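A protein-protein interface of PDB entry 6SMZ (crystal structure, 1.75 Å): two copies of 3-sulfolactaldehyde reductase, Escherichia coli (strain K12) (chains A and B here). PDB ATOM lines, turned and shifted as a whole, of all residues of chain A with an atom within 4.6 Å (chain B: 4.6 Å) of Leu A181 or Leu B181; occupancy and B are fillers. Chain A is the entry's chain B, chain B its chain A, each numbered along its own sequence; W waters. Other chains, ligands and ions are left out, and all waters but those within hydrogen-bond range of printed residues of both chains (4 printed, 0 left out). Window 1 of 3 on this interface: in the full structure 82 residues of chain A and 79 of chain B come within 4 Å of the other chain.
Met A177 touches Ser B185, and with the chains exchanged Ser A185 touches Met B177. Ser A178 touches Ala B211, and with the chains exchanged Ala A211 touches Ser B178. Leu A181 touches His B215, and with the chains exchanged His A215 touches Leu B181. Asn A182 touches His B215, and with the chains exchanged His A215 touches Asn B182. Positions printed for both chains: 177, 178, 179, 180, 181, 182, 183, 184, 185, 210, 211, 214 and 215.
Leu A181 touches just these residues of chain B: Met B177 (3.7 Å), Leu B181 (3.5 Å), Leu B184 (3.5 Å), Ala B210 (3.3 Å), Ala B211 (3.7 Å) and His B215 (3.9 Å). Printed residues of chain A within 4 Å of Leu B181: Met A177 (3.6 Å), Leu A181 (3.5 Å), Leu A184 (3.5 Å), Ala A210 (3.3 Å), Ala A211 (3.8 Å), Gly A214 (3.99 Å) and His A215 (3.9 Å). Of the printed residues of chain B, Asn A182 touches His B215. Of the printed residues of chain A, Ser B178 touches Ala A211 and His A215. Ala A183 touches none of the printed residues of chain B. Gly B214 touches none of the printed residues of chain A. The nearest residue of chain B that does not touch Leu A181 is Gly B214 (4.05 Å). The nearest printed residue of chain A that does not touch Leu B181 is Ser A185 (6.9 Å). The nearest printed residue of chain A that does not touch Ser B185 is His A215 (4.4 Å).
Met A177 touches Leu B184. Ala B211 touches Ser A178 (N to CB, 3.7 Å). Leu B184 touches Ala A180 (CD1 to CB, 3.7 Å). Ala B210 touches Leu A181. Asn A182 touches His B215. CG of Leu A184 touches SD of Met B177, at 3.9 Å. Leu A184 touches Leu B181. O of Ala A210 touches CD2 of Leu B181, at 3.3 Å. Met B177 touches Ala A211 (CG to O, 3.8 Å). Leu B181 touches His A215.
The backbone carbonyl oxygen (O) of Ser B178 lies within hydrogen-bond range of a ring nitrogen (NE2) of His A215. The backbone carbonyl oxygen (O) of Ser A178 sits at hydrogen-bond distance from a ring nitrogen (NE2) of His B215 (2.7 Å).
Hydrophobic or aromatic side chains of chain B within 4 Å of the printed part of chain A: Met B177, Ala B180, Leu B181, Leu B184, Ala B211 and His B215. Of the 13 printed residues of chain A, 11 touch a printed residue of chain B.
O of Leu B181 lies within hydrogen-bond range of OG of Ser B185 (2.8 Å). The backbone carbonyl oxygen of Leu A181 lies within hydrogen-bond range of the side-chain hydroxyl of Ser A185 (2.8 Å).
Water W2 lies within hydrogen-bond range of N of His B215 and OG of Ser A185. Water W3 lies within hydrogen-bond range of OG of Ser B185 and N of His A215. Water W4 bridges the side-chain amide oxygen (OD1) of Asn A182 (3.2 Å) and a ring nitrogen (ND1) of His B215 (3.4 Å). Water W1 bridges a ring nitrogen (ND1) of His A215 (3.2 Å) and the side-chain amide oxygen (OD1) of Asn B182 (3.2 Å).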
ATOM      1  N   MET A 177     -14.033  29.807  26.878  1.00  0.00           N
ATOM      2  CA  MET A 177     -13.898  28.733  25.870  1.00  0.00           C
ATOM      3  C   MET A 177     -12.716  29.027  24.947  1.00  0.00           C
ATOM      4  O   MET A 177     -11.882  28.136  24.731  1.00  0.00           O
ATOM      5  CB  MET A 177     -15.191  28.569  25.071  1.00  0.00           C
ATOM      6  CG  MET A 177     -15.158  27.474  24.062  1.00  0.00           C
ATOM      7  SD  MET A 177     -15.095  25.846  24.923  1.00  0.00           S
ATOM      8  CE  MET A 177     -14.557  24.747  23.622  1.00  0.00           C
ATOM      9  N   SER A 178     -12.598  30.231  24.383  1.00  0.00           N
ATOM     10  CA  SER A 178     -11.569  30.476  23.356  1.00  0.00           C
ATOM     11  C   SER A 178     -10.205  30.469  24.036  1.00  0.00           C
ATOM     12  O   SER A 178      -9.255  29.958  23.440  1.00  0.00           O
ATOM     13  CB  SER A 178     -11.833  31.757  22.567  1.00  0.00           C
ATOM     14  OG  SER A 178     -11.768  32.856  23.447  1.00  0.00           O
ATOM     15  N   ILE A 179     -10.086  31.032  25.244  1.00  0.00           N
ATOM     16  CA  ILE A 179      -8.750  31.166  25.883  1.00  0.00           C
ATOM     17  C   ILE A 179      -8.268  29.744  26.223  1.00  0.00           C
ATOM     18  O   ILE A 179      -7.130  29.445  25.943  1.00  0.00           O
ATOM     19  CB  ILE A 179      -8.811  32.068  27.113  1.00  0.00           C
ATOM     20  CG1 ILE A 179      -9.144  33.502  26.689  1.00  0.00           C
ATOM     21  CG2 ILE A 179      -7.515  32.053  27.863  1.00  0.00           C
ATOM     22  CD1 ILE A 179      -9.599  34.400  27.799  1.00  0.00           C
ATOM     23  N   ALA A 180      -9.111  28.922  26.839  1.00  0.00           N
ATOM     24  CA  ALA A 180      -8.700  27.548  27.217  1.00  0.00           C
ATOM     25  C   ALA A 180      -8.473  26.720  25.949  1.00  0.00           C
ATOM     26  O   ALA A 180      -7.505  25.937  25.893  1.00  0.00           O
ATOM     27  CB  ALA A 180      -9.738  26.946  28.127  1.00  0.00           C
ATOM     28  N   LEU A 181      -9.336  26.869  24.938  1.00  0.00           N
ATOM     29  CA  LEU A 181      -9.241  26.106  23.663  1.00  0.00           C
ATOM     30  C   LEU A 181      -7.864  26.336  23.016  1.00  0.00           C
ATOM     31  O   LEU A 181      -7.295  25.427  22.416  1.00  0.00           O
ATOM     32  CB  LEU A 181     -10.338  26.538  22.708  1.00  0.00           C
ATOM     33  CG  LEU A 181     -10.310  25.905  21.320  1.00  0.00           C
ATOM     34  CD1 LEU A 181     -10.380  24.406  21.424  1.00  0.00           C
ATOM     35  CD2 LEU A 181     -11.476  26.411  20.503  1.00  0.00           C
ATOM     36  N   ASN A 182      -7.309  27.535  23.137  1.00  0.00           N
ATOM     37  CA  ASN A 182      -5.977  27.863  22.580  1.00  0.00           C
ATOM     38  C   ASN A 182      -4.914  26.921  23.161  1.00  0.00           C
ATOM     39  O   ASN A 182      -4.016  26.457  22.432  1.00  0.00           O
ATOM     40  CB  ASN A 182      -5.700  29.352  22.822  1.00  0.00           C
ATOM     41  CG  ASN A 182      -4.440  29.852  22.165  1.00  0.00           C
ATOM     42  OD1 ASN A 182      -4.136  29.480  21.028  1.00  0.00           O
ATOM     43  ND2 ASN A 182      -3.688  30.687  22.894  1.00  0.00           N
ATOM     44  N   ALA A 183      -4.932  26.691  24.478  1.00  0.00           N
ATOM     45  CA  ALA A 183      -3.934  25.828  25.153  1.00  0.00           C
ATOM     46  C   ALA A 183      -4.100  24.390  24.643  1.00  0.00           C
ATOM     47  O   ALA A 183      -3.071  23.743  24.456  1.00  0.00           O
ATOM     48  CB  ALA A 183      -4.051  25.887  26.649  1.00  0.00           C
ATOM     49  N   LEU A 184      -5.344  23.924  24.470  1.00  0.00           N
ATOM     50  CA  LEU A 184      -5.589  22.539  24.001  1.00  0.00           C
ATOM     51  C   LEU A 184      -5.105  22.436  22.552  1.00  0.00           C
ATOM     52  O   LEU A 184      -4.427  21.467  22.187  1.00  0.00           O
ATOM     53  CB  LEU A 184      -7.075  22.207  24.110  1.00  0.00           C
ATOM     54  CG  LEU A 184      -7.429  20.852  23.501  1.00  0.00           C
ATOM     55  CD1 LEU A 184      -6.618  19.741  24.165  1.00  0.00           C
ATOM     56  CD2 LEU A 184      -8.912  20.624  23.612  1.00  0.00           C
ATOM     57  N   SER A 185      -5.457  23.420  21.743  1.00  0.00           N
ATOM     58  CA  SER A 185      -5.065  23.483  20.317  1.00  0.00           C
ATOM     59  C   SER A 185      -3.552  23.352  20.211  1.00  0.00           C
ATOM     60  O   SER A 185      -3.055  22.615  19.348  1.00  0.00           O
ATOM     61  CB  SER A 185      -5.602  24.761  19.695  1.00  0.00           C
ATOM     62  OG  SER A 185      -7.013  24.825  19.741  1.00  0.00           O
ATOM     63  N   ALA A 210     -15.581  17.191  14.596  1.00  0.00           N
ATOM     64  CA  ALA A 210     -15.812  18.029  15.790  1.00  0.00           C
ATOM     65  C   ALA A 210     -14.476  18.648  16.223  1.00  0.00           C
ATOM     66  O   ALA A 210     -14.538  19.660  16.945  1.00  0.00           O
ATOM     67  CB  ALA A 210     -16.419  17.234  16.923  1.00  0.00           C
ATOM     68  N   ALA A 211     -13.328  18.090  15.853  1.00  0.00           N
ATOM     69  CA  ALA A 211     -12.005  18.605  16.275  1.00  0.00           C
ATOM     70  C   ALA A 211     -11.889  20.057  15.811  1.00  0.00           C
ATOM     71  O   ALA A 211     -11.409  20.901  16.586  1.00  0.00           O
ATOM     72  CB  ALA A 211     -10.855  17.793  15.739  1.00  0.00           C
ATOM     73  N   GLY A 214     -15.989  21.964  16.340  1.00  0.00           N
ATOM     74  CA  GLY A 214     -16.578  21.947  17.680  1.00  0.00           C
ATOM     75  C   GLY A 214     -17.721  20.933  17.828  1.00  0.00           C
ATOM     76  O   GLY A 214     -18.284  20.473  16.817  1.00  0.00           O
ATOM     77  N   HIS A 215     -18.049  20.613  19.078  1.00  0.00           N
ATOM     78  CA  HIS A 215     -19.116  19.668  19.469  1.00  0.00           C
ATOM     79  C   HIS A 215     -20.472  20.376  19.536  1.00  0.00           C
ATOM     80  O   HIS A 215     -21.481  19.688  19.409  1.00  0.00           O
ATOM     81  CB  HIS A 215     -18.772  19.022  20.817  1.00  0.00           C
ATOM     82  CG  HIS A 215     -17.629  18.083  20.714  1.00  0.00           C
ATOM     83  ND1 HIS A 215     -17.797  16.767  20.314  1.00  0.00           N
ATOM     84  CD2 HIS A 215     -16.300  18.277  20.872  1.00  0.00           C
ATOM     85  CE1 HIS A 215     -16.609  16.198  20.239  1.00  0.00           C
ATOM     86  NE2 HIS A 215     -15.669  17.103  20.617  1.00  0.00           N
ATOM     87  N   MET B 177      -7.687  15.739  19.689  1.00  0.00           N
ATOM     88  CA  MET B 177      -8.313  17.074  19.717  1.00  0.00           C
ATOM     89  C   MET B 177      -9.802  16.971  20.006  1.00  0.00           C
ATOM     90  O   MET B 177     -10.274  17.681  20.927  1.00  0.00           O
ATOM     91  CB  MET B 177      -8.045  17.821  18.415  1.00  0.00           C
ATOM     92  CG  MET B 177      -8.573  19.224  18.424  1.00  0.00           C
ATOM     93  SD  MET B 177      -7.613  20.253  19.602  1.00  0.00           S
ATOM     94  CE  MET B 177      -8.751  21.639  19.671  1.00  0.00           C
ATOM     95  N   SER B 178     -10.556  16.140  19.286  1.00  0.00           N
ATOM     96  CA  SER B 178     -12.025  16.122  19.469  1.00  0.00           C
ATOM     97  C   SER B 178     -12.350  15.563  20.857  1.00  0.00           C
ATOM     98  O   SER B 178     -13.274  16.066  21.494  1.00  0.00           O
ATOM     99  CB  SER B 178     -12.745  15.336  18.379  1.00  0.00           C
ATOM    100  OG  SER B 178     -12.320  14.007  18.387  1.00  0.00           O
ATOM    101  N   ILE B 179     -11.634  14.535  21.318  1.00  0.00           N
ATOM    102  CA  ILE B 179     -12.003  13.882  22.598  1.00  0.00           C
ATOM    103  C   ILE B 179     -11.730  14.863  23.735  1.00  0.00           C
ATOM    104  O   ILE B 179     -12.610  15.037  24.584  1.00  0.00           O
ATOM    105  CB  ILE B 179     -11.264  12.552  22.750  1.00  0.00           C
ATOM    106  CG1 ILE B 179     -11.709  11.549  21.679  1.00  0.00           C
ATOM    107  CG2 ILE B 179     -11.466  11.983  24.147  1.00  0.00           C
ATOM    108  CD1 ILE B 179     -10.747  10.431  21.533  1.00  0.00           C
ATOM    109  N   ALA B 180     -10.574  15.521  23.736  1.00  0.00           N
ATOM    110  CA  ALA B 180     -10.244  16.496  24.805  1.00  0.00           C
ATOM    111  C   ALA B 180     -11.174  17.709  24.695  1.00  0.00           C
ATOM    112  O   ALA B 180     -11.649  18.214  25.734  1.00  0.00           O
ATOM    113  CB  ALA B 180      -8.792  16.865  24.718  1.00  0.00           C
ATOM    114  N   LEU B 181     -11.447  18.179  23.473  1.00  0.00           N
ATOM    115  CA  LEU B 181     -12.323  19.361  23.242  1.00  0.00           C
ATOM    116  C   LEU B 181     -13.709  19.144  23.851  1.00  0.00           C
ATOM    117  O   LEU B 181     -14.308  20.099  24.395  1.00  0.00           O
ATOM    118  CB  LEU B 181     -12.431  19.618  21.745  1.00  0.00           C
ATOM    119  CG  LEU B 181     -13.370  20.756  21.353  1.00  0.00           C
ATOM    120  CD1 LEU B 181     -12.900  22.058  21.975  1.00  0.00           C
ATOM    121  CD2 LEU B 181     -13.401  20.867  19.839  1.00  0.00           C
ATOM    122  N   ASN B 182     -14.215  17.916  23.820  1.00  0.00           N
ATOM    123  CA  ASN B 182     -15.536  17.588  24.395  1.00  0.00           C
ATOM    124  C   ASN B 182     -15.546  17.947  25.895  1.00  0.00           C
ATOM    125  O   ASN B 182     -16.566  18.493  26.403  1.00  0.00           O
ATOM    126  CB  ASN B 182     -15.836  16.122  24.070  1.00  0.00           C
ATOM    127  CG  ASN B 182     -17.209  15.667  24.508  1.00  0.00           C
ATOM    128  OD1 ASN B 182     -18.191  16.401  24.343  1.00  0.00           O
ATOM    129  ND2 ASN B 182     -17.271  14.466  25.066  1.00  0.00           N
ATOM    130  N   ALA B 183     -14.502  17.584  26.643  1.00  0.00           N
ATOM    131  CA  ALA B 183     -14.447  17.847  28.091  1.00  0.00           C
ATOM    132  C   ALA B 183     -14.387  19.365  28.325  1.00  0.00           C
ATOM    133  O   ALA B 183     -15.046  19.827  29.267  1.00  0.00           O
ATOM    134  CB  ALA B 183     -13.257  17.143  28.721  1.00  0.00           C
ATOM    135  N   LEU B 184     -13.629  20.113  27.530  1.00  0.00           N
ATOM    136  CA  LEU B 184     -13.545  21.589  27.696  1.00  0.00           C
ATOM    137  C   LEU B 184     -14.913  22.204  27.373  1.00  0.00           C
ATOM    138  O   LEU B 184     -15.407  23.059  28.125  1.00  0.00           O
ATOM    139  CB  LEU B 184     -12.480  22.187  26.789  1.00  0.00           C
ATOM    140  CG  LEU B 184     -12.428  23.713  26.832  1.00  0.00           C
ATOM    141  CD1 LEU B 184     -12.184  24.187  28.261  1.00  0.00           C
ATOM    142  CD2 LEU B 184     -11.386  24.255  25.880  1.00  0.00           C
ATOM    143  N   SER B 185     -15.510  21.762  26.274  1.00  0.00           N
ATOM    144  CA  SER B 185     -16.854  22.222  25.833  1.00  0.00           C
ATOM    145  C   SER B 185     -17.860  22.053  26.962  1.00  0.00           C
ATOM    146  O   SER B 185     -18.659  22.975  27.203  1.00  0.00           O
ATOM    147  CB  SER B 185     -17.268  21.485  24.588  1.00  0.00           C
ATOM    148  OG  SER B 185     -16.354  21.731  23.529  1.00  0.00           O
ATOM    149  N   ALA B 210     -13.229  32.260  17.712  1.00  0.00           N
ATOM    150  CA  ALA B 210     -12.354  31.077  17.879  1.00  0.00           C
ATOM    151  C   ALA B 210     -13.002  30.062  18.832  1.00  0.00           C
ATOM    152  O   ALA B 210     -12.626  28.882  18.726  1.00  0.00           O
ATOM    153  CB  ALA B 210     -10.974  31.462  18.367  1.00  0.00           C
ATOM    154  N   ALA B 211     -13.890  30.484  19.730  1.00  0.00           N
ATOM    155  CA  ALA B 211     -14.502  29.583  20.737  1.00  0.00           C
ATOM    156  C   ALA B 211     -15.228  28.449  20.000  1.00  0.00           C
ATOM    157  O   ALA B 211     -15.106  27.279  20.420  1.00  0.00           O
ATOM    158  CB  ALA B 211     -15.449  30.286  21.668  1.00  0.00           C
ATOM    159  N   GLY B 214     -12.664  27.457  16.305  1.00  0.00           N
ATOM    160  CA  GLY B 214     -11.275  27.001  16.502  1.00  0.00           C
ATOM    161  C   GLY B 214     -10.256  28.094  16.213  1.00  0.00           C
ATOM    162  O   GLY B 214     -10.593  29.040  15.488  1.00  0.00           O
ATOM    163  N   HIS B 215      -9.050  27.952  16.763  1.00  0.00           N
ATOM    164  CA  HIS B 215      -7.885  28.844  16.552  1.00  0.00           C
ATOM    165  C   HIS B 215      -7.124  28.486  15.281  1.00  0.00           C
ATOM    166  O   HIS B 215      -6.460  29.366  14.731  1.00  0.00           O
ATOM    167  CB  HIS B 215      -6.934  28.779  17.750  1.00  0.00           C
ATOM    168  CG  HIS B 215      -7.517  29.395  18.958  1.00  0.00           C
ATOM    169  ND1 HIS B 215      -7.439  30.750  19.188  1.00  0.00           N
ATOM    170  CD2 HIS B 215      -8.227  28.866  19.974  1.00  0.00           C
ATOM    171  CE1 HIS B 215      -8.087  31.040  20.306  1.00  0.00           C
ATOM    172  NE2 HIS B 215      -8.571  29.897  20.822  1.00  0.00           N
HETATM  173  O   HOH W   1     -19.589  14.728  21.997  1.00  0.00           O
HETATM  174  O   HOH W   2      -8.783  25.389  17.634  1.00  0.00           O
HETATM  175  O   HOH W   3     -16.906  22.392  20.895  1.00  0.00           O
HETATM  176  O   HOH W   4      -4.367  32.267  19.563  1.00  0.00           O
